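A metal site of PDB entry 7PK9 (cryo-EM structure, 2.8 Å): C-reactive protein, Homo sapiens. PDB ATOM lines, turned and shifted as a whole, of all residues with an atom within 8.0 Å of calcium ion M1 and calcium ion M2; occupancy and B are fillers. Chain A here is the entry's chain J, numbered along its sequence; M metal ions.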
ATOM      1  N   SER A  50      -2.240 -12.829  -1.947  1.00  0.00           N
ATOM      2  CA  SER A  50      -3.319 -13.472  -2.698  1.00  0.00           C
ATOM      3  C   SER A  50      -4.200 -12.470  -3.415  1.00  0.00           C
ATOM      4  O   SER A  50      -4.767 -11.569  -2.790  1.00  0.00           O
ATOM      5  CB  SER A  50      -4.170 -14.327  -1.778  1.00  0.00           C
ATOM      6  OG  SER A  50      -5.286 -14.828  -2.496  1.00  0.00           O
ATOM      7  N   SER A  53      -8.662 -16.288  -4.560  1.00  0.00           N
ATOM      8  CA  SER A  53      -8.589 -17.601  -3.930  1.00  0.00           C
ATOM      9  C   SER A  53      -9.915 -18.342  -4.103  1.00  0.00           C
ATOM     10  O   SER A  53     -10.941 -17.933  -3.548  1.00  0.00           O
ATOM     11  CB  SER A  53      -8.253 -17.463  -2.453  1.00  0.00           C
ATOM     12  OG  SER A  53      -8.057 -18.724  -1.845  1.00  0.00           O
ATOM     13  N   TYR A  54      -9.885 -19.413  -4.875  1.00  0.00           N
ATOM     14  CA  TYR A  54     -11.014 -20.284  -5.147  1.00  0.00           C
ATOM     15  C   TYR A  54     -10.737 -21.632  -4.513  1.00  0.00           C
ATOM     16  O   TYR A  54      -9.881 -22.375  -4.986  1.00  0.00           O
ATOM     17  CB  TYR A  54     -11.206 -20.391  -6.662  1.00  0.00           C
ATOM     18  CG  TYR A  54     -12.361 -21.205  -7.171  1.00  0.00           C
ATOM     19  CD1 TYR A  54     -12.389 -22.577  -7.016  1.00  0.00           C
ATOM     20  CD2 TYR A  54     -13.414 -20.605  -7.833  1.00  0.00           C
ATOM     21  CE1 TYR A  54     -13.426 -23.321  -7.509  1.00  0.00           C
ATOM     22  CE2 TYR A  54     -14.448 -21.334  -8.327  1.00  0.00           C
ATOM     23  CZ  TYR A  54     -14.457 -22.696  -8.168  1.00  0.00           C
ATOM     24  OH  TYR A  54     -15.502 -23.437  -8.655  1.00  0.00           O
ATOM     25  N   ALA A  55     -11.439 -21.952  -3.428  1.00  0.00           N
ATOM     26  CA  ALA A  55     -11.207 -23.171  -2.679  1.00  0.00           C
ATOM     27  C   ALA A  55     -12.434 -24.064  -2.705  1.00  0.00           C
ATOM     28  O   ALA A  55     -13.526 -23.628  -2.326  1.00  0.00           O
ATOM     29  CB  ALA A  55     -10.836 -22.846  -1.225  1.00  0.00           C
ATOM     30  N   GLN A  59      -9.789 -29.116  -2.060  1.00  0.00           N
ATOM     31  CA  GLN A  59      -8.550 -28.438  -2.448  1.00  0.00           C
ATOM     32  C   GLN A  59      -8.689 -26.947  -2.173  1.00  0.00           C
ATOM     33  O   GLN A  59      -9.490 -26.274  -2.808  1.00  0.00           O
ATOM     34  CB  GLN A  59      -8.231 -28.689  -3.910  1.00  0.00           C
ATOM     35  CG  GLN A  59      -6.931 -28.067  -4.369  1.00  0.00           C
ATOM     36  CD  GLN A  59      -5.723 -28.662  -3.701  1.00  0.00           C
ATOM     37  OE1 GLN A  59      -5.633 -29.868  -3.516  1.00  0.00           O
ATOM     38  NE2 GLN A  59      -4.791 -27.812  -3.311  1.00  0.00           N
ATOM     39  N   ASP A  60      -7.902 -26.443  -1.212  1.00  0.00           N
ATOM     40  CA  ASP A  60      -7.951 -25.036  -0.848  1.00  0.00           C
ATOM     41  C   ASP A  60      -7.353 -24.127  -1.918  1.00  0.00           C
ATOM     42  O   ASP A  60      -7.665 -22.933  -1.934  1.00  0.00           O
ATOM     43  CB  ASP A  60      -7.194 -24.811   0.464  1.00  0.00           C
ATOM     44  CG  ASP A  60      -5.730 -25.198   0.364  1.00  0.00           C
ATOM     45  OD1 ASP A  60      -5.431 -26.395   0.166  1.00  0.00           O
ATOM     46  OD2 ASP A  60      -4.872 -24.306   0.489  1.00  0.00           O
ATOM     47  N   ASN A  61      -6.497 -24.661  -2.792  1.00  0.00           N
ATOM     48  CA  ASN A  61      -5.923 -23.887  -3.878  1.00  0.00           C
ATOM     49  C   ASN A  61      -6.470 -24.368  -5.219  1.00  0.00           C
ATOM     50  O   ASN A  61      -5.705 -24.740  -6.108  1.00  0.00           O
ATOM     51  CB  ASN A  61      -4.403 -23.978  -3.872  1.00  0.00           C
ATOM     52  CG  ASN A  61      -3.793 -23.360  -2.637  1.00  0.00           C
ATOM     53  OD1 ASN A  61      -4.484 -22.743  -1.829  1.00  0.00           O
ATOM     54  ND2 ASN A  61      -2.482 -23.504  -2.498  1.00  0.00           N
ATOM     55  N   GLU A  62      -7.793 -24.409  -5.341  1.00  0.00           N
ATOM     56  CA  GLU A  62      -8.408 -24.964  -6.536  1.00  0.00           C
ATOM     57  C   GLU A  62      -8.272 -24.023  -7.741  1.00  0.00           C
ATOM     58  O   GLU A  62      -7.992 -24.479  -8.842  1.00  0.00           O
ATOM     59  CB  GLU A  62      -9.872 -25.263  -6.240  1.00  0.00           C
ATOM     60  CG  GLU A  62     -10.637 -25.876  -7.377  1.00  0.00           C
ATOM     61  CD  GLU A  62     -10.135 -27.251  -7.715  1.00  0.00           C
ATOM     62  OE1 GLU A  62      -9.575 -27.918  -6.837  1.00  0.00           O
ATOM     63  OE2 GLU A  62     -10.307 -27.656  -8.872  1.00  0.00           O
ATOM     64  N   LEU A  64      -5.946 -20.394  -7.817  1.00  0.00           N
ATOM     65  CA  LEU A  64      -5.252 -19.334  -7.097  1.00  0.00           C
ATOM     66  C   LEU A  64      -4.391 -18.534  -8.036  1.00  0.00           C
ATOM     67  O   LEU A  64      -3.543 -19.093  -8.734  1.00  0.00           O
ATOM     68  CB  LEU A  64      -4.399 -19.916  -5.978  1.00  0.00           C
ATOM     69  CG  LEU A  64      -3.855 -18.894  -4.995  1.00  0.00           C
ATOM     70  CD1 LEU A  64      -4.955 -18.198  -4.245  1.00  0.00           C
ATOM     71  CD2 LEU A  64      -2.916 -19.574  -4.035  1.00  0.00           C
ATOM     72  N   PHE A  66      -1.659 -15.741  -7.531  1.00  0.00           N
ATOM     73  CA  PHE A  66      -0.851 -15.263  -6.422  1.00  0.00           C
ATOM     74  C   PHE A  66       0.326 -14.479  -6.977  1.00  0.00           C
ATOM     75  O   PHE A  66       1.112 -15.018  -7.752  1.00  0.00           O
ATOM     76  CB  PHE A  66      -0.386 -16.433  -5.556  1.00  0.00           C
ATOM     77  CG  PHE A  66       0.058 -16.044  -4.183  1.00  0.00           C
ATOM     78  CD1 PHE A  66      -0.844 -15.943  -3.153  1.00  0.00           C
ATOM     79  CD2 PHE A  66       1.395 -15.848  -3.925  1.00  0.00           C
ATOM     80  CE1 PHE A  66      -0.417 -15.604  -1.892  1.00  0.00           C
ATOM     81  CE2 PHE A  66       1.814 -15.509  -2.675  1.00  0.00           C
ATOM     82  CZ  PHE A  66       0.915 -15.394  -1.647  1.00  0.00           C
ATOM     83  N   THR A  76      -2.246 -21.118 -10.237  1.00  0.00           N
ATOM     84  CA  THR A  76      -2.384 -22.521  -9.870  1.00  0.00           C
ATOM     85  C   THR A  76      -3.815 -23.006 -10.027  1.00  0.00           C
ATOM     86  O   THR A  76      -4.765 -22.305  -9.672  1.00  0.00           O
ATOM     87  CB  THR A  76      -1.976 -22.784  -8.420  1.00  0.00           C
ATOM     88  OG1 THR A  76      -3.064 -22.471  -7.561  1.00  0.00           O
ATOM     89  CG2 THR A  76      -0.825 -21.921  -8.026  1.00  0.00           C
ATOM     90  N   GLN A 137      -7.932 -12.330   0.862  1.00  0.00           N
ATOM     91  CA  GLN A 137      -7.210 -13.266   1.700  1.00  0.00           C
ATOM     92  C   GLN A 137      -6.794 -14.473   0.871  1.00  0.00           C
ATOM     93  O   GLN A 137      -7.297 -14.721  -0.213  1.00  0.00           O
ATOM     94  CB  GLN A 137      -8.042 -13.744   2.893  1.00  0.00           C
ATOM     95  CG  GLN A 137      -8.444 -12.659   3.844  1.00  0.00           C
ATOM     96  CD  GLN A 137      -7.265 -12.075   4.583  1.00  0.00           C
ATOM     97  OE1 GLN A 137      -6.210 -12.693   4.667  1.00  0.00           O
ATOM     98  NE2 GLN A 137      -7.440 -10.880   5.117  1.00  0.00           N
ATOM     99  N   GLU A 138      -5.858 -15.224   1.443  1.00  0.00           N
ATOM    100  CA  GLU A 138      -5.508 -16.556   0.997  1.00  0.00           C
ATOM    101  C   GLU A 138      -6.089 -17.548   1.982  1.00  0.00           C
ATOM    102  O   GLU A 138      -5.844 -17.452   3.184  1.00  0.00           O
ATOM    103  CB  GLU A 138      -3.995 -16.724   0.935  1.00  0.00           C
ATOM    104  CG  GLU A 138      -3.549 -18.079   0.455  1.00  0.00           C
ATOM    105  CD  GLU A 138      -3.946 -18.321  -0.942  1.00  0.00           C
ATOM    106  OE1 GLU A 138      -4.097 -17.318  -1.654  1.00  0.00           O
ATOM    107  OE2 GLU A 138      -4.099 -19.499  -1.327  1.00  0.00           O
ATOM    108  N   GLN A 139      -6.840 -18.506   1.462  1.00  0.00           N
ATOM    109  CA  GLN A 139      -7.474 -19.508   2.302  1.00  0.00           C
ATOM    110  C   GLN A 139      -6.753 -20.835   2.116  1.00  0.00           C
ATOM    111  O   GLN A 139      -6.553 -21.278   0.985  1.00  0.00           O
ATOM    112  CB  GLN A 139      -8.962 -19.589   1.999  1.00  0.00           C
ATOM    113  CG  GLN A 139      -9.354 -20.282   0.747  1.00  0.00           C
ATOM    114  CD  GLN A 139     -10.697 -19.802   0.253  1.00  0.00           C
ATOM    115  OE1 GLN A 139     -11.728 -20.146   0.807  1.00  0.00           O
ATOM    116  NE2 GLN A 139     -10.686 -19.032  -0.815  1.00  0.00           N
ATOM    117  N   ASP A 140      -6.352 -21.447   3.227  1.00  0.00           N
ATOM    118  CA  ASP A 140      -5.689 -22.736   3.246  1.00  0.00           C
ATOM    119  C   ASP A 140      -6.608 -23.860   3.692  1.00  0.00           C
ATOM    120  O   ASP A 140      -6.224 -25.035   3.608  1.00  0.00           O
ATOM    121  CB  ASP A 140      -4.467 -22.673   4.177  1.00  0.00           C
ATOM    122  CG  ASP A 140      -3.312 -21.917   3.567  1.00  0.00           C
ATOM    123  OD1 ASP A 140      -2.596 -21.216   4.296  1.00  0.00           O
ATOM    124  OD2 ASP A 140      -3.108 -22.023   2.330  1.00  0.00           O
ATOM    125  N   SER A 141      -7.804 -23.532   4.162  1.00  0.00           N
ATOM    126  CA  SER A 141      -8.870 -24.480   4.367  1.00  0.00           C
ATOM    127  C   SER A 141     -10.113 -23.890   3.723  1.00  0.00           C
ATOM    128  O   SER A 141     -10.152 -22.693   3.399  1.00  0.00           O
ATOM    129  CB  SER A 141      -9.112 -24.779   5.850  1.00  0.00           C
ATOM    130  OG  SER A 141      -9.607 -23.662   6.548  1.00  0.00           O
ATOM    131  N   GLY A 144     -11.298 -20.562   5.129  1.00  0.00           N
ATOM    132  CA  GLY A 144     -10.667 -20.187   6.381  1.00  0.00           C
ATOM    133  C   GLY A 144      -9.167 -20.356   6.354  1.00  0.00           C
ATOM    134  O   GLY A 144      -8.555 -20.551   5.304  1.00  0.00           O
ATOM    135  N   ASN A 145      -8.588 -20.258   7.550  1.00  0.00           N
ATOM    136  CA  ASN A 145      -7.138 -20.325   7.734  1.00  0.00           C
ATOM    137  C   ASN A 145      -6.420 -19.259   6.916  1.00  0.00           C
ATOM    138  O   ASN A 145      -5.456 -19.541   6.187  1.00  0.00           O
ATOM    139  CB  ASN A 145      -6.607 -21.720   7.409  1.00  0.00           C
ATOM    140  CG  ASN A 145      -7.149 -22.770   8.329  1.00  0.00           C
ATOM    141  OD1 ASN A 145      -7.984 -22.481   9.185  1.00  0.00           O
ATOM    142  ND2 ASN A 145      -6.666 -23.999   8.192  1.00  0.00           N
ATOM    143  N   PHE A 146      -6.902 -18.032   7.019  1.00  0.00           N
ATOM    144  CA  PHE A 146      -6.256 -16.914   6.365  1.00  0.00           C
ATOM    145  C   PHE A 146      -4.926 -16.593   7.029  1.00  0.00           C
ATOM    146  O   PHE A 146      -4.707 -16.870   8.214  1.00  0.00           O
ATOM    147  CB  PHE A 146      -7.163 -15.693   6.399  1.00  0.00           C
ATOM    148  CG  PHE A 146      -8.539 -15.976   5.887  1.00  0.00           C
ATOM    149  CD1 PHE A 146      -8.732 -16.570   4.667  1.00  0.00           C
ATOM    150  CD2 PHE A 146      -9.648 -15.633   6.634  1.00  0.00           C
ATOM    151  CE1 PHE A 146      -9.991 -16.815   4.198  1.00  0.00           C
ATOM    152  CE2 PHE A 146     -10.906 -15.885   6.172  1.00  0.00           C
ATOM    153  CZ  PHE A 146     -11.077 -16.477   4.946  1.00  0.00           C
ATOM    154  N   GLU A 147      -4.019 -16.006   6.238  1.00  0.00           N
ATOM    155  CA  GLU A 147      -2.735 -15.517   6.736  1.00  0.00           C
ATOM    156  C   GLU A 147      -2.578 -14.064   6.324  1.00  0.00           C
ATOM    157  O   GLU A 147      -2.677 -13.739   5.146  1.00  0.00           O
ATOM    158  CB  GLU A 147      -1.579 -16.365   6.198  1.00  0.00           C
ATOM    159  CG  GLU A 147      -1.720 -17.854   6.485  1.00  0.00           C
ATOM    160  CD  GLU A 147      -0.456 -18.646   6.168  1.00  0.00           C
ATOM    161  OE1 GLU A 147      -0.424 -19.363   5.155  1.00  0.00           O
ATOM    162  OE2 GLU A 147       0.513 -18.529   6.950  1.00  0.00           O
ATOM    163  N   GLY A 148      -2.317 -13.202   7.306  1.00  0.00           N
ATOM    164  CA  GLY A 148      -2.190 -11.782   7.024  1.00  0.00           C
ATOM    165  C   GLY A 148      -1.082 -11.465   6.037  1.00  0.00           C
ATOM    166  O   GLY A 148      -1.235 -10.607   5.164  1.00  0.00           O
ATOM    167  N   SER A 149       0.055 -12.147   6.156  1.00  0.00           N
ATOM    168  CA  SER A 149       1.159 -11.969   5.234  1.00  0.00           C
ATOM    169  C   SER A 149       0.809 -12.354   3.797  1.00  0.00           C
ATOM    170  O   SER A 149       1.647 -12.226   2.909  1.00  0.00           O
ATOM    171  CB  SER A 149       2.372 -12.779   5.706  1.00  0.00           C
ATOM    172  OG  SER A 149       2.114 -14.174   5.649  1.00  0.00           O
ATOM    173  N   GLN A 150      -0.404 -12.856   3.566  1.00  0.00           N
ATOM    174  CA  GLN A 150      -0.905 -13.115   2.223  1.00  0.00           C
ATOM    175  C   GLN A 150      -2.155 -12.315   1.861  1.00  0.00           C
ATOM    176  O   GLN A 150      -2.663 -12.464   0.751  1.00  0.00           O
ATOM    177  CB  GLN A 150      -1.177 -14.607   2.093  1.00  0.00           C
ATOM    178  CG  GLN A 150       0.097 -15.413   2.206  1.00  0.00           C
ATOM    179  CD  GLN A 150      -0.065 -16.876   1.865  1.00  0.00           C
ATOM    180  OE1 GLN A 150      -1.089 -17.470   2.153  1.00  0.00           O
ATOM    181  NE2 GLN A 150       0.961 -17.449   1.267  1.00  0.00           N
HETATM  182 CA    CA M   1      -3.874 -21.912   0.234  1.00  0.00          CA
HETATM  183 CA    CA M   2      -1.744 -19.519   2.997  1.00  0.00          CA
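N of Ser 50 sits at hydrogen-bond distance from O of Gln 150 (2.8 Å).
OG of Ser 53 lies within hydrogen-bond range of NE2 of Gln 139, at 2.8 Å.
The side-chain carboxylate of Glu 138 lies within hydrogen-bond range of the side-chain hydroxyl of Ser 50, at 2.9 Å.
Of the 23 residues printed, 5 come within 4 Å of calcium ion M1.
The nearest printed residue that does not touch calcium ion M1 is Leu 64 (5.0 Å).
Four residues have an atom within 4 Å of calcium ion M2: Glu 138, Asp 140, Glu 147 and Gln 150.
Calcium ion M1 is bound by the side-chain carboxylate (OD2) of Asp 140, the side-chain amide oxygen (OD1) of Asn 61, the side-chain carboxylate (OD2) of Asp 60, the backbone carbonyl oxygen (O) of Gln 139 and the side-chain carboxylate (OE2) of Glu 138.
OD1 of Asp 140 is bound to calcium ion M2 (2.3 Å).
OE1 of Gln 150 is bound to calcium ion M2, 2.3 Å away.
The side-chain carboxylate (OE1) of Glu 147 binds calcium ion M2 (2.5 Å).
Calcium ion M2 has three donor atoms within binding distance.
Slightly farther from calcium ion M2 lies the side-chain carboxylate (OD2) of Asp 140 (2.9 Å).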
